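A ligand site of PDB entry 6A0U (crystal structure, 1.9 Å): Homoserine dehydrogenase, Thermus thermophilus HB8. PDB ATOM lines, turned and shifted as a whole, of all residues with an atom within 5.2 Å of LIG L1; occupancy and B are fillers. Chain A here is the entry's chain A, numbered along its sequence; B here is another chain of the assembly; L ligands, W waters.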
ATOM      1  N   GLY A  10      -5.780  -9.855 -22.472  1.00  0.00           N
ATOM      2  CA  GLY A  10      -6.573 -10.027 -21.296  1.00  0.00           C
ATOM      3  C   GLY A  10      -7.735  -9.034 -21.305  1.00  0.00           C
ATOM      4  O   GLY A  10      -7.530  -7.863 -21.630  1.00  0.00           O
ATOM      5  N   GLY A  11      -8.916  -9.516 -20.961  1.00  0.00           N
ATOM      6  CA  GLY A  11     -10.144  -8.788 -20.930  1.00  0.00           C
ATOM      7  C   GLY A  11     -10.933  -9.075 -19.715  1.00  0.00           C
ATOM      8  O   GLY A  11     -12.180  -9.031 -19.685  1.00  0.00           O
ATOM      9  N   GLY A  12     -10.190  -9.318 -18.628  1.00  0.00           N
ATOM     10  CA  GLY A  12     -10.820  -9.723 -17.399  1.00  0.00           C
ATOM     11  C   GLY A  12     -11.049  -8.627 -16.406  1.00  0.00           C
ATOM     12  O   GLY A  12     -11.465  -7.474 -16.723  1.00  0.00           O
ATOM     13  N   THR A  13     -10.849  -8.981 -15.166  1.00  0.00           N
ATOM     14  CA  THR A  13     -11.087  -7.985 -14.085  1.00  0.00           C
ATOM     15  C   THR A  13     -10.246  -6.679 -14.371  1.00  0.00           C
ATOM     16  O   THR A  13     -10.771  -5.560 -14.361  1.00  0.00           O
ATOM     17  CB  THR A  13     -10.732  -8.563 -12.708  1.00  0.00           C
ATOM     18  OG1 THR A  13     -11.783  -9.433 -12.279  1.00  0.00           O
ATOM     19  CG2 THR A  13     -10.678  -7.439 -11.638  1.00  0.00           C
ATOM     20  N   VAL A  14      -9.003  -6.882 -14.707  1.00  0.00           N
ATOM     21  CA  VAL A  14      -8.127  -5.747 -14.966  1.00  0.00           C
ATOM     22  C   VAL A  14      -8.346  -5.236 -16.387  1.00  0.00           C
ATOM     23  O   VAL A  14      -8.537  -4.020 -16.601  1.00  0.00           O
ATOM     24  CB  VAL A  14      -6.646  -6.148 -14.787  1.00  0.00           C
ATOM     25  CG1 VAL A  14      -5.733  -5.090 -15.299  1.00  0.00           C
ATOM     26  CG2 VAL A  14      -6.334  -6.515 -13.313  1.00  0.00           C
ATOM     27  N   GLY A  15      -8.275  -6.133 -17.366  1.00  0.00           N
ATOM     28  CA  GLY A  15      -8.380  -5.768 -18.782  1.00  0.00           C
ATOM     29  C   GLY A  15      -9.611  -5.014 -19.183  1.00  0.00           C
ATOM     30  O   GLY A  15      -9.559  -4.018 -19.964  1.00  0.00           O
ATOM     31  N   LEU A  42      -7.285  -9.962 -26.583  1.00  0.00           N
ATOM     32  CA  LEU A  42      -7.104 -11.444 -26.366  1.00  0.00           C
ATOM     33  C   LEU A  42      -7.798 -11.905 -25.202  1.00  0.00           C
ATOM     34  O   LEU A  42      -7.628 -11.415 -24.067  1.00  0.00           O
ATOM     35  CB  LEU A  42      -5.646 -11.846 -26.261  1.00  0.00           C
ATOM     36  CG  LEU A  42      -5.362 -13.390 -26.321  1.00  0.00           C
ATOM     37  CD1 LEU A  42      -5.646 -13.900 -27.730  1.00  0.00           C
ATOM     38  CD2 LEU A  42      -3.899 -13.607 -26.047  1.00  0.00           C
ATOM     39  N   VAL A  43      -8.669 -12.888 -25.415  1.00  0.00           N
ATOM     40  CA  VAL A  43      -9.450 -13.499 -24.360  1.00  0.00           C
ATOM     41  C   VAL A  43      -9.558 -15.064 -24.602  1.00  0.00           C
ATOM     42  O   VAL A  43      -9.118 -15.568 -25.629  1.00  0.00           O
ATOM     43  CB  VAL A  43     -10.880 -12.946 -24.212  1.00  0.00           C
ATOM     44  CG1 VAL A  43     -10.857 -11.407 -24.070  1.00  0.00           C
ATOM     45  CG2 VAL A  43     -11.767 -13.320 -25.427  1.00  0.00           C
ATOM     46  N   ARG A  44      -9.968 -15.745 -23.580  1.00  0.00           N
ATOM     47  CA  ARG A  44     -10.071 -17.244 -23.592  1.00  0.00           C
ATOM     48  C   ARG A  44     -11.407 -17.641 -24.194  1.00  0.00           C
ATOM     49  O   ARG A  44     -11.465 -18.486 -25.127  1.00  0.00           O
ATOM     50  CB  ARG A  44      -9.995 -17.830 -22.207  1.00  0.00           C
ATOM     51  CG  ARG A  44      -8.568 -17.837 -21.729  1.00  0.00           C
ATOM     52  CD  ARG A  44      -8.339 -18.424 -20.342  1.00  0.00           C
ATOM     53  NE  ARG A  44      -9.030 -17.733 -19.230  1.00  0.00           N
ATOM     54  CZ  ARG A  44      -8.651 -17.765 -17.938  1.00  0.00           C
ATOM     55  NH1 ARG A  44      -7.560 -18.404 -17.549  1.00  0.00           N
ATOM     56  NH2 ARG A  44      -9.348 -17.131 -17.035  1.00  0.00           N
ATOM     57  N   ASP A  45     -12.435 -16.997 -23.670  1.00  0.00           N
ATOM     58  CA  ASP A  45     -13.814 -17.321 -23.891  1.00  0.00           C
ATOM     59  C   ASP A  45     -14.602 -16.159 -24.505  1.00  0.00           C
ATOM     60  O   ASP A  45     -15.198 -15.410 -23.824  1.00  0.00           O
ATOM     61  CB  ASP A  45     -14.433 -17.795 -22.597  1.00  0.00           C
ATOM     62  CG  ASP A  45     -15.903 -18.258 -22.799  1.00  0.00           C
ATOM     63  OD1 ASP A  45     -16.516 -18.676 -21.803  1.00  0.00           O
ATOM     64  OD2 ASP A  45     -16.437 -18.192 -23.947  1.00  0.00           O
ATOM     65  N   PRO A  46     -14.669 -16.076 -25.826  1.00  0.00           N
ATOM     66  CA  PRO A  46     -15.290 -14.905 -26.452  1.00  0.00           C
ATOM     67  C   PRO A  46     -16.793 -14.854 -26.250  1.00  0.00           C
ATOM     68  O   PRO A  46     -17.429 -13.871 -26.624  1.00  0.00           O
ATOM     69  CB  PRO A  46     -14.860 -14.999 -27.927  1.00  0.00           C
ATOM     70  CG  PRO A  46     -14.631 -16.458 -28.157  1.00  0.00           C
ATOM     71  CD  PRO A  46     -14.270 -17.091 -26.824  1.00  0.00           C
ATOM     72  N   LYS A  48     -18.278 -15.143 -23.051  1.00  0.00           N
ATOM     73  CA  LYS A  48     -18.750 -14.592 -21.767  1.00  0.00           C
ATOM     74  C   LYS A  48     -19.222 -13.131 -21.976  1.00  0.00           C
ATOM     75  O   LYS A  48     -18.632 -12.407 -22.804  1.00  0.00           O
ATOM     76  CB  LYS A  48     -17.659 -14.548 -20.728  1.00  0.00           C
ATOM     77  CG  LYS A  48     -17.211 -15.904 -20.239  1.00  0.00           C
ATOM     78  CD  LYS A  48     -15.797 -15.856 -19.652  1.00  0.00           C
ATOM     79  CE  LYS A  48     -15.638 -14.851 -18.531  1.00  0.00           C
ATOM     80  NZ  LYS A  48     -16.708 -15.008 -17.500  1.00  0.00           N
ATOM     81  N   ARG A  50     -19.163  -9.458 -21.540  1.00  0.00           N
ATOM     82  CA  ARG A  50     -17.944  -8.691 -21.328  1.00  0.00           C
ATOM     83  C   ARG A  50     -18.257  -7.268 -21.724  1.00  0.00           C
ATOM     84  O   ARG A  50     -18.841  -7.083 -22.774  1.00  0.00           O
ATOM     85  CB  ARG A  50     -16.858  -9.264 -22.217  1.00  0.00           C
ATOM     86  CG  ARG A  50     -15.431  -9.054 -21.730  1.00  0.00           C
ATOM     87  CD  ARG A  50     -14.395  -9.531 -22.726  1.00  0.00           C
ATOM     88  NE  ARG A  50     -14.429 -11.009 -22.847  1.00  0.00           N
ATOM     89  CZ  ARG A  50     -13.917 -11.901 -21.980  1.00  0.00           C
ATOM     90  NH1 ARG A  50     -13.243 -11.530 -20.881  1.00  0.00           N
ATOM     91  NH2 ARG A  50     -14.048 -13.217 -22.233  1.00  0.00           N
ATOM     92  N   GLU A  72      -0.656  -5.725 -21.299  1.00  0.00           N
ATOM     93  CA  GLU A  72      -0.877  -7.131 -20.867  1.00  0.00           C
ATOM     94  C   GLU A  72      -1.409  -7.212 -19.501  1.00  0.00           C
ATOM     95  O   GLU A  72      -0.897  -6.585 -18.514  1.00  0.00           O
ATOM     96  CB  GLU A  72       0.425  -7.934 -21.033  1.00  0.00           C
ATOM     97  CG  GLU A  72       0.242  -9.446 -20.666  1.00  0.00           C
ATOM     98  CD  GLU A  72       0.469  -9.740 -19.222  1.00  0.00           C
ATOM     99  OE1 GLU A  72       1.513  -9.269 -18.707  1.00  0.00           O
ATOM    100  OE2 GLU A  72      -0.358 -10.412 -18.631  1.00  0.00           O
ATOM    101  N   ALA A  73      -2.496  -7.966 -19.358  1.00  0.00           N
ATOM    102  CA  ALA A  73      -3.061  -8.296 -18.114  1.00  0.00           C
ATOM    103  C   ALA A  73      -3.817  -9.676 -18.213  1.00  0.00           C
ATOM    104  O   ALA A  73      -5.019  -9.801 -17.898  1.00  0.00           O
ATOM    105  CB  ALA A  73      -4.066  -7.289 -17.708  1.00  0.00           C
ATOM    106  N   MET A  74      -3.055 -10.670 -18.624  1.00  0.00           N
ATOM    107  CA  MET A  74      -3.627 -12.034 -18.869  1.00  0.00           C
ATOM    108  C   MET A  74      -3.234 -13.007 -17.743  1.00  0.00           C
ATOM    109  O   MET A  74      -4.039 -13.925 -17.391  1.00  0.00           O
ATOM    110  CB  MET A  74      -3.335 -12.503 -20.308  1.00  0.00           C
ATOM    111  CG  MET A  74      -1.924 -12.739 -20.638  1.00  0.00           C
ATOM    112  SD  MET A  74      -1.621 -13.199 -22.319  1.00  0.00           S
ATOM    113  CE  MET A  74      -2.347 -14.857 -22.267  1.00  0.00           C
ATOM    114  N   GLY A  75      -2.105 -12.796 -17.088  1.00  0.00           N
ATOM    115  CA  GLY A  75      -1.731 -13.764 -16.057  1.00  0.00           C
ATOM    116  C   GLY A  75      -0.809 -14.782 -16.643  1.00  0.00           C
ATOM    117  O   GLY A  75      -0.692 -14.903 -17.869  1.00  0.00           O
ATOM    118  N   GLY A  76      -0.001 -15.408 -15.763  1.00  0.00           N
ATOM    119  CA  GLY A  76       0.905 -16.469 -16.203  1.00  0.00           C
ATOM    120  C   GLY A  76       2.187 -15.883 -16.617  1.00  0.00           C
ATOM    121  O   GLY A  76       2.473 -14.689 -16.408  1.00  0.00           O
ATOM    122  N   ALA A  79       3.093 -17.956 -21.560  1.00  0.00           N
ATOM    123  CA  ALA A  79       2.219 -17.558 -22.675  1.00  0.00           C
ATOM    124  C   ALA A  79       2.313 -16.045 -22.987  1.00  0.00           C
ATOM    125  O   ALA A  79       2.711 -15.685 -24.079  1.00  0.00           O
ATOM    126  CB  ALA A  79       0.825 -17.933 -22.357  1.00  0.00           C
ATOM    127  N   ALA A  97       0.716  -5.363 -15.869  1.00  0.00           N
ATOM    128  CA  ALA A  97       0.416  -5.504 -14.487  1.00  0.00           C
ATOM    129  C   ALA A  97       0.866  -6.905 -13.915  1.00  0.00           C
ATOM    130  O   ALA A  97       0.556  -7.208 -12.790  1.00  0.00           O
ATOM    131  CB  ALA A  97      -1.050  -5.283 -14.226  1.00  0.00           C
ATOM    132  N   ASN A  98       1.683  -7.601 -14.649  1.00  0.00           N
ATOM    133  CA  ASN A  98       1.930  -9.053 -14.335  1.00  0.00           C
ATOM    134  C   ASN A  98       3.289  -9.234 -13.662  1.00  0.00           C
ATOM    135  O   ASN A  98       4.325  -9.266 -14.300  1.00  0.00           O
ATOM    136  CB  ASN A  98       1.966  -9.765 -15.664  1.00  0.00           C
ATOM    137  CG  ASN A  98       1.985 -11.303 -15.473  1.00  0.00           C
ATOM    138  OD1 ASN A  98       2.416 -11.813 -14.444  1.00  0.00           O
ATOM    139  ND2 ASN A  98       1.520 -12.022 -16.496  1.00  0.00           N
ATOM    140  N   LYS A  99       3.274  -9.338 -12.368  1.00  0.00           N
ATOM    141  CA  LYS A  99       4.548  -9.415 -11.592  1.00  0.00           C
ATOM    142  C   LYS A  99       5.201 -10.792 -11.714  1.00  0.00           C
ATOM    143  O   LYS A  99       6.444 -10.916 -11.758  1.00  0.00           O
ATOM    144  CB  LYS A  99       4.331  -9.083 -10.139  1.00  0.00           C
ATOM    145  CG  LYS A  99       3.542 -10.042  -9.309  1.00  0.00           C
ATOM    146  CD  LYS A  99       3.357  -9.653  -7.866  1.00  0.00           C
ATOM    147  CE  LYS A  99       2.165  -8.767  -7.546  1.00  0.00           C
ATOM    148  NZ  LYS A  99       0.842  -9.321  -7.997  1.00  0.00           N
ATOM    149  N   ALA A 122       1.639  -0.885 -12.441  1.00  0.00           N
ATOM    150  CA  ALA A 122       0.514  -1.720 -11.936  1.00  0.00           C
ATOM    151  C   ALA A 122       0.893  -3.121 -11.464  1.00  0.00           C
ATOM    152  O   ALA A 122       0.047  -3.816 -10.844  1.00  0.00           O
ATOM    153  CB  ALA A 122      -0.665  -1.798 -12.988  1.00  0.00           C
ATOM    154  N   ALA A 126      -0.684  -2.296  -7.523  1.00  0.00           N
ATOM    155  CA  ALA A 126      -1.683  -1.794  -8.453  1.00  0.00           C
ATOM    156  C   ALA A 126      -1.379  -0.291  -8.821  1.00  0.00           C
ATOM    157  O   ALA A 126      -0.233   0.033  -9.039  1.00  0.00           O
ATOM    158  CB  ALA A 126      -3.037  -1.988  -7.920  1.00  0.00           C
ATOM    159  N   GLY A 177     -12.020  -9.633  -6.414  1.00  0.00           N
ATOM    160  CA  GLY A 177     -11.159  -9.606  -7.612  1.00  0.00           C
ATOM    161  C   GLY A 177      -9.707  -9.362  -7.198  1.00  0.00           C
ATOM    162  O   GLY A 177      -8.849  -9.194  -8.066  1.00  0.00           O
ATOM    163  N   TYR A 178      -9.432  -9.394  -5.895  1.00  0.00           N
ATOM    164  CA  TYR A 178      -8.012  -9.326  -5.410  1.00  0.00           C
ATOM    165  C   TYR A 178      -7.002 -10.499  -5.700  1.00  0.00           C
ATOM    166  O   TYR A 178      -5.792 -10.217  -5.921  1.00  0.00           O
ATOM    167  CB  TYR A 178      -7.972  -9.122  -3.911  1.00  0.00           C
ATOM    168  CG  TYR A 178      -8.706  -7.941  -3.428  1.00  0.00           C
ATOM    169  CD1 TYR A 178      -9.112  -6.890  -4.320  1.00  0.00           C
ATOM    170  CD2 TYR A 178      -9.011  -7.817  -2.094  1.00  0.00           C
ATOM    171  CE1 TYR A 178      -9.898  -5.822  -3.854  1.00  0.00           C
ATOM    172  CE2 TYR A 178      -9.783  -6.796  -1.636  1.00  0.00           C
ATOM    173  CZ  TYR A 178     -10.181  -5.788  -2.494  1.00  0.00           C
ATOM    174  OH  TYR A 178     -10.850  -4.734  -1.993  1.00  0.00           O
ATOM    175  N   ALA A 179      -7.474 -11.778  -5.699  1.00  0.00           N
ATOM    176  CA  ALA A 179      -6.582 -12.917  -5.476  1.00  0.00           C
ATOM    177  C   ALA A 179      -6.052 -13.312  -6.733  1.00  0.00           C
ATOM    178  O   ALA A 179      -6.626 -13.079  -7.794  1.00  0.00           O
ATOM    179  CB  ALA A 179      -7.313 -14.045  -4.718  1.00  0.00           C
ATOM    180  N   GLU A 180      -4.852 -13.835  -6.722  1.00  0.00           N
ATOM    181  CA  GLU A 180      -4.370 -14.381  -7.905  1.00  0.00           C
ATOM    182  C   GLU A 180      -5.378 -15.596  -8.203  1.00  0.00           C
ATOM    183  O   GLU A 180      -6.179 -15.999  -7.327  1.00  0.00           O
ATOM    184  CB  GLU A 180      -2.908 -14.872  -7.806  1.00  0.00           C
ATOM    185  CG  GLU A 180      -1.867 -13.724  -7.634  1.00  0.00           C
ATOM    186  CD  GLU A 180      -2.045 -12.700  -8.750  1.00  0.00           C
ATOM    187  OE1 GLU A 180      -2.622 -11.698  -8.412  1.00  0.00           O
ATOM    188  OE2 GLU A 180      -1.612 -12.960  -9.922  1.00  0.00           O
ATOM    189  N   ASP A 191       3.337 -14.314  -4.241  1.00  0.00           N
ATOM    190  CA  ASP A 191       2.988 -13.134  -4.982  1.00  0.00           C
ATOM    191  C   ASP A 191       3.786 -11.870  -4.397  1.00  0.00           C
ATOM    192  O   ASP A 191       4.372 -11.118  -5.150  1.00  0.00           O
ATOM    193  CB  ASP A 191       1.498 -12.918  -4.866  1.00  0.00           C
ATOM    194  CG  ASP A 191       1.015 -11.680  -5.677  1.00  0.00           C
ATOM    195  OD1 ASP A 191       0.885 -10.642  -4.996  1.00  0.00           O
ATOM    196  OD2 ASP A 191       0.898 -11.764  -6.938  1.00  0.00           O
ATOM    197  N   GLY A 288      -3.971  -1.992  -3.168  1.00  0.00           N
ATOM    198  CA  GLY A 288      -2.946  -2.814  -3.868  1.00  0.00           C
ATOM    199  C   GLY A 288      -3.423  -3.915  -4.799  1.00  0.00           C
ATOM    200  O   GLY A 288      -2.575  -4.645  -5.420  1.00  0.00           O
ATOM    201  N   ALA A 289      -4.735  -3.925  -4.993  1.00  0.00           N
ATOM    202  CA  ALA A 289      -5.389  -4.908  -5.797  1.00  0.00           C
ATOM    203  C   ALA A 289      -6.779  -4.349  -6.138  1.00  0.00           C
ATOM    204  O   ALA A 289      -7.236  -3.427  -5.473  1.00  0.00           O
ATOM    205  CB  ALA A 289      -5.548  -6.218  -4.975  1.00  0.00           C
ATOM    206  N   GLY A 290      -7.443  -4.934  -7.159  1.00  0.00           N
ATOM    207  CA  GLY A 290      -8.771  -4.454  -7.615  1.00  0.00           C
ATOM    208  C   GLY A 290      -8.665  -4.049  -9.099  1.00  0.00           C
ATOM    209  O   GLY A 290      -7.589  -3.606  -9.557  1.00  0.00           O
ATOM    210  N   GLY A 291      -9.747  -4.241  -9.858  1.00  0.00           N
ATOM    211  CA  GLY A 291      -9.730  -3.870 -11.248  1.00  0.00           C
ATOM    212  C   GLY A 291      -9.423  -2.395 -11.599  1.00  0.00           C
ATOM    213  O   GLY A 291      -8.480  -2.144 -12.374  1.00  0.00           O
ATOM    214  N   THR A 294      -5.975  -1.285 -10.458  1.00  0.00           N
ATOM    215  CA  THR A 294      -5.013  -1.678 -11.391  1.00  0.00           C
ATOM    216  C   THR A 294      -5.071  -0.961 -12.714  1.00  0.00           C
ATOM    217  O   THR A 294      -4.003  -0.583 -13.296  1.00  0.00           O
ATOM    218  CB  THR A 294      -5.096  -3.246 -11.586  1.00  0.00           C
ATOM    219  OG1 THR A 294      -5.065  -3.867 -10.310  1.00  0.00           O
ATOM    220  CG2 THR A 294      -4.027  -3.737 -12.292  1.00  0.00           C
ATOM    221  N   ALA B 167       0.909 -20.776 -27.242  1.00  0.00           N
ATOM    222  CA  ALA B 167      -0.147 -19.894 -26.700  1.00  0.00           C
ATOM    223  C   ALA B 167      -1.469 -20.264 -27.289  1.00  0.00           C
ATOM    224  O   ALA B 167      -2.465 -20.343 -26.572  1.00  0.00           O
ATOM    225  CB  ALA B 167       0.199 -18.427 -27.046  1.00  0.00           C
ATOM    226  N   LEU B 170      -2.454 -23.492 -25.501  1.00  0.00           N
ATOM    227  CA  LEU B 170      -2.864 -23.350 -24.115  1.00  0.00           C
ATOM    228  C   LEU B 170      -4.212 -22.700 -23.982  1.00  0.00           C
ATOM    229  O   LEU B 170      -4.998 -22.986 -23.045  1.00  0.00           O
ATOM    230  CB  LEU B 170      -1.873 -22.486 -23.315  1.00  0.00           C
ATOM    231  CG  LEU B 170      -2.302 -21.981 -21.951  1.00  0.00           C
ATOM    232  CD1 LEU B 170      -2.587 -23.061 -20.907  1.00  0.00           C
ATOM    233  CD2 LEU B 170      -1.192 -21.061 -21.443  1.00  0.00           C
ATOM    234  N   LEU B 171      -4.409 -21.735 -24.873  1.00  0.00           N
ATOM    235  CA  LEU B 171      -5.682 -21.034 -24.930  1.00  0.00           C
ATOM    236  C   LEU B 171      -6.694 -22.102 -25.213  1.00  0.00           C
ATOM    237  O   LEU B 171      -7.625 -22.359 -24.386  1.00  0.00           O
ATOM    238  CB  LEU B 171      -5.599 -19.983 -26.042  1.00  0.00           C
ATOM    239  CG  LEU B 171      -6.345 -18.711 -25.741  1.00  0.00           C
ATOM    240  CD1 LEU B 171      -5.857 -17.668 -26.745  1.00  0.00           C
ATOM    241  CD2 LEU B 171      -7.854 -18.976 -25.816  1.00  0.00           C
ATOM    242  N   GLN B 174      -7.337 -24.293 -22.252  1.00  0.00           N
ATOM    243  CA  GLN B 174      -8.133 -23.691 -21.178  1.00  0.00           C
ATOM    244  C   GLN B 174      -9.669 -23.613 -21.575  1.00  0.00           C
ATOM    245  O   GLN B 174     -10.505 -23.803 -20.745  1.00  0.00           O
ATOM    246  CB  GLN B 174      -7.654 -22.274 -20.848  1.00  0.00           C
ATOM    247  CG  GLN B 174      -6.420 -22.267 -20.027  1.00  0.00           C
ATOM    248  CD  GLN B 174      -5.817 -20.884 -19.930  1.00  0.00           C
ATOM    249  OE1 GLN B 174      -5.243 -20.350 -20.921  1.00  0.00           O
ATOM    250  NE2 GLN B 174      -5.844 -20.354 -18.791  1.00  0.00           N
HETATM  251  P1  LIG L   1      -8.783 -12.350 -14.801  1.00  0.00           P
HETATM  252  O1  LIG L   1      -8.681 -13.847 -14.806  1.00  0.00           O
HETATM  253  O2  LIG L   1      -9.958 -11.644 -14.320  1.00  0.00           O
HETATM  254  O3  LIG L   1      -8.492 -11.980 -16.341  1.00  0.00           O
HETATM  255  C1  LIG L   1      -7.610 -12.768 -17.160  1.00  0.00           C
HETATM  256  C2  LIG L   1      -7.879 -12.371 -18.597  1.00  0.00           C
HETATM  257  O4  LIG L   1      -6.929 -12.962 -19.498  1.00  0.00           O
HETATM  258  C3  LIG L   1      -9.240 -12.895 -19.032  1.00  0.00           C
HETATM  259  O5  LIG L   1      -9.848 -12.050 -20.019  1.00  0.00           O
HETATM  260  C4  LIG L   1      -8.944 -14.267 -19.664  1.00  0.00           C
HETATM  261  O6  LIG L   1      -9.865 -14.599 -20.707  1.00  0.00           O
HETATM  262  C5  LIG L   1      -7.581 -14.023 -20.273  1.00  0.00           C
HETATM  263  N1  LIG L   1      -6.695 -15.178 -20.278  1.00  0.00           N
HETATM  264  C6  LIG L   1      -6.201 -15.848 -19.177  1.00  0.00           C
HETATM  265  N2  LIG L   1      -5.260 -16.736 -19.623  1.00  0.00           N
HETATM  266  C7  LIG L   1      -5.205 -16.681 -20.986  1.00  0.00           C
HETATM  267  C8  LIG L   1      -4.491 -17.364 -22.111  1.00  0.00           C
HETATM  268  N3  LIG L   1      -3.595 -18.348 -21.931  1.00  0.00           N
HETATM  269  N4  LIG L   1      -4.717 -16.948 -23.373  1.00  0.00           N
HETATM  270  C9  LIG L   1      -5.574 -15.927 -23.646  1.00  0.00           C
HETATM  271  N5  LIG L   1      -6.292 -15.272 -22.705  1.00  0.00           N
HETATM  272  C10 LIG L   1      -6.136 -15.589 -21.380  1.00  0.00           C
HETATM  273  O7  LIG L   1      -7.352 -11.929 -14.099  1.00  0.00           O
HETATM  274  P2  LIG L   1      -6.979 -10.360 -13.673  1.00  0.00           P
HETATM  275  O8  LIG L   1      -7.484 -10.060 -12.355  1.00  0.00           O
HETATM  276  O9  LIG L   1      -7.559  -9.426 -14.751  1.00  0.00           O
HETATM  277  O10 LIG L   1      -5.375 -10.453 -13.682  1.00  0.00           O
HETATM  278  C11 LIG L   1      -4.636 -10.333 -14.837  1.00  0.00           C
HETATM  279  C12 LIG L   1      -3.277  -9.932 -14.411  1.00  0.00           C
HETATM  280  O11 LIG L   1      -3.420  -8.730 -13.705  1.00  0.00           O
HETATM  281  C13 LIG L   1      -2.621 -10.986 -13.479  1.00  0.00           C
HETATM  282  O12 LIG L   1      -1.307 -11.025 -14.044  1.00  0.00           O
HETATM  283  C14 LIG L   1      -2.643 -10.440 -12.112  1.00  0.00           C
HETATM  284  O13 LIG L   1      -1.501 -10.937 -11.416  1.00  0.00           O
HETATM  285  C15 LIG L   1      -2.576  -8.930 -12.541  1.00  0.00           C
HETATM  286  N6  LIG L   1      -3.071  -8.083 -11.523  1.00  0.00           N
HETATM  287  C16 LIG L   1      -4.299  -8.259 -10.992  1.00  0.00           C
HETATM  288  C17 LIG L   1      -4.704  -7.439  -9.998  1.00  0.00           C
HETATM  289  C18 LIG L   1      -6.014  -7.621  -9.390  1.00  0.00           C
HETATM  290  O14 LIG L   1      -6.204  -7.078  -8.326  1.00  0.00           O
HETATM  291  N7  LIG L   1      -6.925  -8.406  -9.968  1.00  0.00           N
HETATM  292  C19 LIG L   1      -3.860  -6.381  -9.532  1.00  0.00           C
HETATM  293  C20 LIG L   1      -2.655  -6.214 -10.143  1.00  0.00           C
HETATM  294  C21 LIG L   1      -2.262  -7.088 -11.118  1.00  0.00           C
HETATM  295  P3  LIG L   1     -11.386 -14.827 -20.209  1.00  0.00           P
HETATM  296  O15 LIG L   1     -11.490 -15.880 -19.171  1.00  0.00           O
HETATM  297  O16 LIG L   1     -12.105 -13.657 -19.453  1.00  0.00           O
HETATM  298  O17 LIG L   1     -11.955 -15.197 -21.584  1.00  0.00           O
HETATM  299  N1  LG2 L   2      -3.192 -10.947  -5.765  1.00  0.00           N
HETATM  300  C1  LG2 L   2      -2.409  -9.651  -5.770  1.00  0.00           C
HETATM  301  C2  LG2 L   2      -2.591  -9.036  -4.405  1.00  0.00           C
HETATM  302  C3  LG2 L   2      -2.719  -8.663  -6.953  1.00  0.00           C
HETATM  303  O1  LG2 L   2      -3.373  -9.583  -3.657  1.00  0.00           O
HETATM  304  O2  LG2 L   2      -1.879  -8.050  -3.982  1.00  0.00           O
HETATM  305  C4  LG2 L   2      -1.938  -7.307  -6.922  1.00  0.00           C
HETATM  306  O3  LG2 L   2      -0.509  -7.367  -6.966  1.00  0.00           O
HETATM  307  O   HOH W   1      -7.712  -8.976 -17.309  1.00  0.00           O
HETATM  308  O   HOH W   2     -13.187 -13.225 -17.229  1.00  0.00           O
HETATM  309  O   HOH W   3      -3.866 -17.883 -17.826  1.00  0.00           O
HETATM  310  O   HOH W   4      -8.298 -14.327 -11.835  1.00  0.00           O
HETATM  311  O   HOH W   5      -6.481 -12.645 -10.626  1.00  0.00           O
HETATM  312  O   HOH W   6      -0.006  -4.960  -8.363  1.00  0.00           O
HETATM  313  O   HOH W   7      -4.900 -10.791  -9.315  1.00  0.00           O
HETATM  314  O   HOH W   8       0.721  -9.216 -11.019  1.00  0.00           O
HETATM  315  O   HOH W   9      -9.310 -11.105 -10.733  1.00  0.00           O
HETATM  316  O   HOH W  10       0.381 -13.250 -13.407  1.00  0.00           O
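Water W3 bridges a nitrogen (N2) of LIG L1 and the side-chain amide nitrogen of Gln 174 of chain B.
Water W1 lies within hydrogen-bond range of O9 of LIG L1 (2.6 Å), N of Gly 12 (2.8 Å), O of Ala 73 (2.9 Å) and N of Gly 15 (2.9 Å).
Water W9 lies within hydrogen-bond range of O8 of LIG L1 (2.7 Å), O of Gly 177 (3.3 Å) and OG1 of Thr 13 (3.4 Å).
Water W7 lies within hydrogen-bond range of the side-chain carboxylate (OE1) of Glu 180 (2.6 Å), a nitrogen (N7) of LIG L1 (3.2 Å) and the backbone carbonyl oxygen (O) of Ala 179 (3.2 Å).
Water W5 bridges the backbone carbonyl oxygen of Ala 179 and an oxygen (O8) of LIG L1.
Water W6 lies within hydrogen-bond range of the backbone carbonyl oxygen of Ala 122 (2.7 Å), an oxygen (O3) of LG2 L2 (2.8 Å) and the backbone NH of Ala 126 (2.9 Å).
The backbone carbonyl oxygen of Gly 76 sits at hydrogen-bond distance from the side-chain amide nitrogen of Asn 98 (2.8 Å).
The backbone NH (N) of Met 74 lies within hydrogen-bond range of the side-chain carboxylate (OE2) of Glu 72 (2.7 Å).
ND2 of Asn 98 sits at hydrogen-bond distance from OE2 of Glu 72, at 3.3 Å.
N of Gly 10 lies within hydrogen-bond range of O of Leu 42, 2.9 Å away.
The side-chain carboxylate (OE2) of Glu 72 lies within hydrogen-bond range of the backbone NH (N) of Gly 75, at 3.3 Å.
O of Glu 72 sits at hydrogen-bond distance from N of Ala 97 (3.3 Å).
The backbone carbonyl oxygen (O) of Gly 290 lies within hydrogen-bond range of the side-chain hydroxyl (OG1) of Thr 294 (2.6 Å).
The side-chain amide oxygen of Gln 174 of chain B lies close to the backbone carbonyl oxygen of Leu 170 of chain B, at 3.4 Å.
Merely in contact with LIG L1: Gly 10, Leu 42, Val 43, Lys 48, Ala 73, Met 74, Gly 75, Ala 97, Asn 98, Ala 122, Tyr 178, Ala 289, Thr 294, Leu 170 of chain B and Leu 171 of chain B.
Hydrophobic or aromatic side chains within 4 Å of LIG L1: Val 14, Leu 42, Val 43, Met 74, Ala 97, Ala 289, Leu 170 of chain B and Leu 171 of chain B.
Of the 38 residues printed, 26 come within 4 Å of LIG L1.
The nearest printed residue that does not touch LIG L1 is Gly 15 (4.3 Å).
The side-chain amino group (NZ) of Lys 99 is in hydrogen-bond range of an oxygen (O3) of LG2 L2.
O16 of LIG L1 is in salt-bridge range of NH1 of Arg 50 (2.8 Å).
The backbone NH (N) of Gly 12 sits at hydrogen-bond distance from an oxygen (O5) of LIG L1 (3.1 Å).
The backbone NH of Asp 45 is in hydrogen-bond range of an oxygen (O17) of LIG L1 (2.8 Å).
O of Tyr 178 sits at hydrogen-bond distance from N1 of LG2 L2 (2.7 Å).
NE of Arg 44 is in salt-bridge range of O15 of LIG L1.
The backbone NH (N) of Thr 13 is in hydrogen-bond range of an oxygen (O2) of LIG L1, 2.9 Å away.
OE1 of Glu 180 lies within salt-bridge range of N1 of LG2 L2 (2.8 Å).
OE1 of Gln 174 of chain B sits at hydrogen-bond distance from N3 of LIG L1, 2.8 Å away.
The backbone NH (N) of Val 14 sits at hydrogen-bond distance from an oxygen (O9) of LIG L1, at 2.9 Å.
A nitrogen (N1) of LG2 L2 sits close to the backbone NH of Glu 180 (3.5 Å).
An oxygen (O14) of LIG L1 sits at hydrogen-bond distance from the backbone NH (N) of Gly 290 (2.7 Å).
The backbone NH (N) of Gly 11 sits at hydrogen-bond distance from an oxygen (O5) of LIG L1, at 2.9 Å.
O of Gly 177 lies within hydrogen-bond range of N7 of LIG L1 (2.8 Å).
The side-chain carboxylate (OE2) of Glu 180 is in hydrogen-bond range of an oxygen (O13) of LIG L1.
An oxygen (O17) of LIG L1 sits at hydrogen-bond distance from the backbone NH (N) of Arg 44 (2.9 Å).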
